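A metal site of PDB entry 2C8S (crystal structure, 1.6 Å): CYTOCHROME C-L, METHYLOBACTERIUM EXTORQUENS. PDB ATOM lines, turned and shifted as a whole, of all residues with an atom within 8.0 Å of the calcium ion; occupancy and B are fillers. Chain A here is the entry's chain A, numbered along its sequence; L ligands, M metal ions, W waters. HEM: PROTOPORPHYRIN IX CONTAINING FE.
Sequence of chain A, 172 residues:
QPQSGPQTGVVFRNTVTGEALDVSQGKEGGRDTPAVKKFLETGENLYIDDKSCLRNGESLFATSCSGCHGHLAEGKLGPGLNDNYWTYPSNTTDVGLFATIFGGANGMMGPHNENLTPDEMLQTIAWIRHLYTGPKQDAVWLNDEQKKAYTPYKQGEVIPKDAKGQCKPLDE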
ATOM      1  N   HIS A  69      24.320   1.425  29.198  1.00  0.00           N
ATOM      2  CA  HIS A  69      23.436   1.757  28.088  1.00  0.00           C
ATOM      3  C   HIS A  69      23.918   2.918  27.232  1.00  0.00           C
ATOM      4  O   HIS A  69      23.306   3.237  26.217  1.00  0.00           O
ATOM      5  CB  HIS A  69      22.039   2.048  28.609  1.00  0.00           C
ATOM      6  CG  HIS A  69      21.327   0.830  29.096  1.00  0.00           C
ATOM      7  ND1 HIS A  69      20.787  -0.107  28.240  1.00  0.00           N
ATOM      8  CD2 HIS A  69      21.127   0.364  30.356  1.00  0.00           C
ATOM      9  CE1 HIS A  69      20.279  -1.094  28.953  1.00  0.00           C
ATOM     10  NE2 HIS A  69      20.464  -0.843  30.240  1.00  0.00           N
ATOM     11  N   ALA A  73      21.871   6.702  26.035  1.00  0.00           N
ATOM     12  CA  ALA A  73      21.041   5.505  25.992  1.00  0.00           C
ATOM     13  C   ALA A  73      21.014   4.926  24.572  1.00  0.00           C
ATOM     14  O   ALA A  73      20.059   4.258  24.165  1.00  0.00           O
ATOM     15  CB  ALA A  73      19.630   5.821  26.458  1.00  0.00           C
ATOM     16  N   GLU A  74      22.096   5.162  23.831  1.00  0.00           N
ATOM     17  CA  GLU A  74      22.213   4.680  22.459  1.00  0.00           C
ATOM     18  C   GLU A  74      22.623   3.205  22.435  1.00  0.00           C
ATOM     19  O   GLU A  74      22.543   2.543  21.391  1.00  0.00           O
ATOM     20  CB  GLU A  74      23.265   5.496  21.701  1.00  0.00           C
ATOM     21  CG  GLU A  74      24.703   5.198  22.137  1.00  0.00           C
ATOM     22  CD  GLU A  74      25.213   6.149  23.210  1.00  0.00           C
ATOM     23  OE1 GLU A  74      24.416   6.601  24.048  1.00  0.00           O
ATOM     24  OE2 GLU A  74      26.435   6.439  23.215  1.00  0.00           O
ATOM     25  N   PRO A  79      21.546  -2.812  25.656  1.00  0.00           N
ATOM     26  CA  PRO A  79      20.894  -2.301  24.451  1.00  0.00           C
ATOM     27  C   PRO A  79      20.549  -0.819  24.430  1.00  0.00           C
ATOM     28  O   PRO A  79      20.554  -0.152  25.467  1.00  0.00           O
ATOM     29  CB  PRO A  79      19.645  -3.167  24.349  1.00  0.00           C
ATOM     30  CG  PRO A  79      19.294  -3.402  25.782  1.00  0.00           C
ATOM     31  CD  PRO A  79      20.648  -3.735  26.370  1.00  0.00           C
ATOM     32  N   GLY A  80      20.263  -0.301  23.242  1.00  0.00           N
ATOM     33  CA  GLY A  80      19.891   1.091  23.121  1.00  0.00           C
ATOM     34  C   GLY A  80      18.451   1.230  23.611  1.00  0.00           C
ATOM     35  O   GLY A  80      17.580   0.463  23.216  1.00  0.00           O
ATOM     36  N   LEU A  81      18.221   2.201  24.474  1.00  0.00           N
ATOM     37  CA  LEU A  81      16.884   2.432  25.015  1.00  0.00           C
ATOM     38  C   LEU A  81      16.256   3.649  24.393  1.00  0.00           C
ATOM     39  O   LEU A  81      15.194   4.094  24.832  1.00  0.00           O
ATOM     40  CB  LEU A  81      16.956   2.627  26.532  1.00  0.00           C
ATOM     41  CG  LEU A  81      17.724   1.561  27.317  1.00  0.00           C
ATOM     42  CD1 LEU A  81      17.795   2.000  28.764  1.00  0.00           C
ATOM     43  CD2 LEU A  81      17.055   0.210  27.208  1.00  0.00           C
ATOM     44  N   ASN A  82      16.899   4.198  23.356  1.00  0.00           N
ATOM     45  CA  ASN A  82      16.424   5.406  22.701  1.00  0.00           C
ATOM     46  C   ASN A  82      15.774   5.170  21.342  1.00  0.00           C
ATOM     47  O   ASN A  82      15.616   6.110  20.571  1.00  0.00           O
ATOM     48  CB  ASN A  82      17.587   6.374  22.504  1.00  0.00           C
ATOM     49  CG  ASN A  82      18.608   5.851  21.511  1.00  0.00           C
ATOM     50  OD1 ASN A  82      18.607   4.666  21.183  1.00  0.00           O
ATOM     51  ND2 ASN A  82      19.473   6.729  21.020  1.00  0.00           N
ATOM     52  N   ASP A  83      15.398   3.931  21.052  1.00  0.00           N
ATOM     53  CA  ASP A  83      14.763   3.630  19.780  1.00  0.00           C
ATOM     54  C   ASP A  83      13.426   2.910  19.953  1.00  0.00           C
ATOM     55  O   ASP A  83      12.986   2.656  21.086  1.00  0.00           O
ATOM     56  CB  ASP A  83      15.700   2.831  18.873  1.00  0.00           C
ATOM     57  CG  ASP A  83      16.162   1.535  19.515  1.00  0.00           C
ATOM     58  OD1 ASP A  83      15.417   0.960  20.335  1.00  0.00           O
ATOM     59  OD2 ASP A  83      17.282   1.085  19.175  1.00  0.00           O
ATOM     60  N   ASN A  84      12.799   2.552  18.838  1.00  0.00           N
ATOM     61  CA  ASN A  84      11.505   1.882  18.903  1.00  0.00           C
ATOM     62  C   ASN A  84      11.514   0.363  18.942  1.00  0.00           C
ATOM     63  O   ASN A  84      10.485  -0.279  18.717  1.00  0.00           O
ATOM     64  CB  ASN A  84      10.602   2.376  17.766  1.00  0.00           C
ATOM     65  CG  ASN A  84      11.012   1.833  16.410  1.00  0.00           C
ATOM     66  OD1 ASN A  84      12.113   1.304  16.241  1.00  0.00           O
ATOM     67  ND2 ASN A  84      10.121   1.964  15.428  1.00  0.00           N
ATOM     68  N   TYR A  85      12.662  -0.243  19.223  1.00  0.00           N
ATOM     69  CA  TYR A  85      12.695  -1.692  19.336  1.00  0.00           C
ATOM     70  C   TYR A  85      12.925  -2.031  20.792  1.00  0.00           C
ATOM     71  O   TYR A  85      13.844  -1.494  21.411  1.00  0.00           O
ATOM     72  CB  TYR A  85      13.819  -2.308  18.507  1.00  0.00           C
ATOM     73  CG  TYR A  85      13.915  -3.789  18.773  1.00  0.00           C
ATOM     74  CD1 TYR A  85      12.899  -4.657  18.353  1.00  0.00           C
ATOM     75  CD2 TYR A  85      14.952  -4.323  19.543  1.00  0.00           C
ATOM     76  CE1 TYR A  85      12.914  -6.003  18.695  1.00  0.00           C
ATOM     77  CE2 TYR A  85      14.974  -5.659  19.892  1.00  0.00           C
ATOM     78  CZ  TYR A  85      13.950  -6.500  19.468  1.00  0.00           C
ATOM     79  OH  TYR A  85      13.962  -7.839  19.816  1.00  0.00           O
ATOM     80  N   TRP A  86      12.091  -2.921  21.331  1.00  0.00           N
ATOM     81  CA  TRP A  86      12.219  -3.355  22.723  1.00  0.00           C
ATOM     82  C   TRP A  86      12.151  -4.876  22.811  1.00  0.00           C
ATOM     83  O   TRP A  86      11.215  -5.480  22.284  1.00  0.00           O
ATOM     84  CB  TRP A  86      11.101  -2.758  23.561  1.00  0.00           C
ATOM     85  CG  TRP A  86      11.035  -1.283  23.500  1.00  0.00           C
ATOM     86  CD1 TRP A  86      10.436  -0.533  22.538  1.00  0.00           C
ATOM     87  CD2 TRP A  86      11.605  -0.355  24.431  1.00  0.00           C
ATOM     88  NE1 TRP A  86      10.592   0.805  22.801  1.00  0.00           N
ATOM     89  CE2 TRP A  86      11.308   0.943  23.964  1.00  0.00           C
ATOM     90  CE3 TRP A  86      12.347  -0.497  25.620  1.00  0.00           C
ATOM     91  CZ2 TRP A  86      11.718   2.092  24.647  1.00  0.00           C
ATOM     92  CZ3 TRP A  86      12.749   0.647  26.288  1.00  0.00           C
ATOM     93  CH2 TRP A  86      12.438   1.931  25.799  1.00  0.00           C
ATOM     94  N   THR A  87      13.133  -5.474  23.467  1.00  0.00           N
ATOM     95  CA  THR A  87      13.144  -6.930  23.628  1.00  0.00           C
ATOM     96  C   THR A  87      11.939  -7.327  24.459  1.00  0.00           C
ATOM     97  O   THR A  87      11.300  -8.351  24.210  1.00  0.00           O
ATOM     98  CB  THR A  87      14.437  -7.393  24.331  1.00  0.00           C
ATOM     99  OG1 THR A  87      15.565  -7.055  23.520  1.00  0.00           O
ATOM    100  CG2 THR A  87      14.409  -8.900  24.536  1.00  0.00           C
ATOM    101  N   TYR A  88      11.632  -6.503  25.452  1.00  0.00           N
ATOM    102  CA  TYR A  88      10.492  -6.717  26.320  1.00  0.00           C
ATOM    103  C   TYR A  88       9.625  -5.481  26.157  1.00  0.00           C
ATOM    104  O   TYR A  88       9.895  -4.430  26.728  1.00  0.00           O
ATOM    105  CB  TYR A  88      10.961  -6.855  27.773  1.00  0.00           C
ATOM    106  CG  TYR A  88      12.056  -7.884  27.937  1.00  0.00           C
ATOM    107  CD1 TYR A  88      11.778  -9.252  27.886  1.00  0.00           C
ATOM    108  CD2 TYR A  88      13.382  -7.494  28.100  1.00  0.00           C
ATOM    109  CE1 TYR A  88      12.798 -10.197  27.977  1.00  0.00           C
ATOM    110  CE2 TYR A  88      14.408  -8.428  28.197  1.00  0.00           C
ATOM    111  CZ  TYR A  88      14.114  -9.773  28.127  1.00  0.00           C
ATOM    112  OH  TYR A  88      15.137 -10.696  28.208  1.00  0.00           O
ATOM    113  N   TYR A 132      14.631   9.527  23.661  1.00  0.00           N
ATOM    114  CA  TYR A 132      14.075   8.833  22.498  1.00  0.00           C
ATOM    115  C   TYR A 132      14.398   9.548  21.187  1.00  0.00           C
ATOM    116  O   TYR A 132      14.410  10.779  21.132  1.00  0.00           O
ATOM    117  CB  TYR A 132      12.547   8.700  22.650  1.00  0.00           C
ATOM    118  CG  TYR A 132      11.854   7.891  21.564  1.00  0.00           C
ATOM    119  CD1 TYR A 132      12.189   6.563  21.323  1.00  0.00           C
ATOM    120  CD2 TYR A 132      10.826   8.460  20.806  1.00  0.00           C
ATOM    121  CE1 TYR A 132      11.513   5.807  20.362  1.00  0.00           C
ATOM    122  CE2 TYR A 132      10.152   7.728  19.849  1.00  0.00           C
ATOM    123  CZ  TYR A 132      10.486   6.395  19.630  1.00  0.00           C
ATOM    124  OH  TYR A 132       9.792   5.658  18.686  1.00  0.00           O
HETATM  125  CHA HEM L   1      18.306  -4.187  29.383  1.00  0.00           C
HETATM  126  CHB HEM L   1      16.898  -0.222  31.745  1.00  0.00           C
HETATM  127  CHC HEM L   1      21.069  -0.282  34.176  1.00  0.00           C
HETATM  128  CHD HEM L   1      22.599  -4.015  31.551  1.00  0.00           C
HETATM  129  C1A HEM L   1      17.537  -3.128  29.850  1.00  0.00           C
HETATM  130  C2A HEM L   1      16.183  -2.866  29.449  1.00  0.00           C
HETATM  131  C3A HEM L   1      15.782  -1.747  30.099  1.00  0.00           C
HETATM  132  C4A HEM L   1      16.897  -1.330  30.908  1.00  0.00           C
HETATM  133  CMA HEM L   1      14.439  -1.038  30.014  1.00  0.00           C
HETATM  134  CAA HEM L   1      15.389  -3.708  28.456  1.00  0.00           C
HETATM  135  CBA HEM L   1      15.433  -3.149  27.040  1.00  0.00           C
HETATM  136  CGA HEM L   1      14.485  -3.813  26.068  1.00  0.00           C
HETATM  137  O1A HEM L   1      13.476  -4.396  26.475  1.00  0.00           O
HETATM  138  O2A HEM L   1      14.723  -3.768  24.865  1.00  0.00           O
HETATM  139  C1B HEM L   1      17.954   0.177  32.565  1.00  0.00           C
HETATM  140  C2B HEM L   1      17.839   1.184  33.572  1.00  0.00           C
HETATM  141  C3B HEM L   1      18.997   1.095  34.313  1.00  0.00           C
HETATM  142  C4B HEM L   1      19.800   0.088  33.715  1.00  0.00           C
HETATM  143  CMB HEM L   1      16.624   2.094  33.730  1.00  0.00           C
HETATM  144  CAB HEM L   1      19.425   1.903  35.557  1.00  0.00           C
HETATM  145  CBB HEM L   1      18.404   2.143  36.667  1.00  0.00           C
HETATM  146  C1C HEM L   1      21.859  -1.302  33.671  1.00  0.00           C
HETATM  147  C2C HEM L   1      23.214  -1.569  34.095  1.00  0.00           C
HETATM  148  C3C HEM L   1      23.636  -2.641  33.363  1.00  0.00           C
HETATM  149  C4C HEM L   1      22.551  -2.969  32.476  1.00  0.00           C
HETATM  150  CMC HEM L   1      23.943  -0.778  35.187  1.00  0.00           C
HETATM  151  CAC HEM L   1      24.910  -3.505  33.507  1.00  0.00           C
HETATM  152  CBC HEM L   1      25.394  -3.931  34.893  1.00  0.00           C
HETATM  153  C1D HEM L   1      21.559  -4.396  30.717  1.00  0.00           C
HETATM  154  C2D HEM L   1      21.623  -5.529  29.825  1.00  0.00           C
HETATM  155  C3D HEM L   1      20.400  -5.591  29.223  1.00  0.00           C
HETATM  156  C4D HEM L   1      19.623  -4.489  29.749  1.00  0.00           C
HETATM  157  CMD HEM L   1      22.819  -6.441  29.645  1.00  0.00           C
HETATM  158  CAD HEM L   1      19.871  -6.638  28.259  1.00  0.00           C
HETATM  159  CBD HEM L   1      19.197  -7.801  28.994  1.00  0.00           C
HETATM  160  CGD HEM L   1      18.300  -8.714  28.155  1.00  0.00           C
HETATM  161  O1D HEM L   1      17.670  -9.614  28.702  1.00  0.00           O
HETATM  162  O2D HEM L   1      18.213  -8.542  26.940  1.00  0.00           O
HETATM  163  NA  HEM L   1      17.975  -2.178  30.758  1.00  0.00           N
HETATM  164  NB  HEM L   1      19.168  -0.491  32.638  1.00  0.00           N
HETATM  165  NC  HEM L   1      21.478  -2.145  32.657  1.00  0.00           N
HETATM  166  ND  HEM L   1      20.344  -3.762  30.669  1.00  0.00           N
HETATM  167 FE   HEM L   1      19.727  -2.127  31.690  1.00  0.00          FE
HETATM  168 CA    CA M   1      15.822  -0.606  22.145  1.00  0.00          CA
HETATM  169  O   HOH W   1      14.407   1.310  23.022  1.00  0.00           O
HETATM  170  O   HOH W   2      15.087  -1.095  24.374  1.00  0.00           O
HETATM  171  O   HOH W   3      17.260  -1.303  20.372  1.00  0.00           O
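N of Thr 87 lies within hydrogen-bond range of O2A of the ligand (2.7 Å).
A ring nitrogen (NE2) of His 69 binds an iron atom (FE) of the ligand, 2.1 Å away.
O1A of the ligand sits at hydrogen-bond distance from N of Tyr 88, at 3.0 Å.
The side-chain hydroxyl of Tyr 88 is in hydrogen-bond range of an oxygen (O1D) of the ligand.
The calcium ion is bound by O of Tyr 85 (2.3 Å), O of Gly 80 (2.3 Å), water W3 (2.4 Å), water W2 (2.4 Å), OD1 of Asp 83 (2.4 Å) and water W1 (2.5 Å).
The nearest printed residue that does not touch the calcium ion is Leu 81 (4.3 Å).
The backbone carbonyl oxygen (O) of Asp 83 is in hydrogen-bond range of the indole nitrogen (NE1) of Trp 86, at 3.5 Å.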
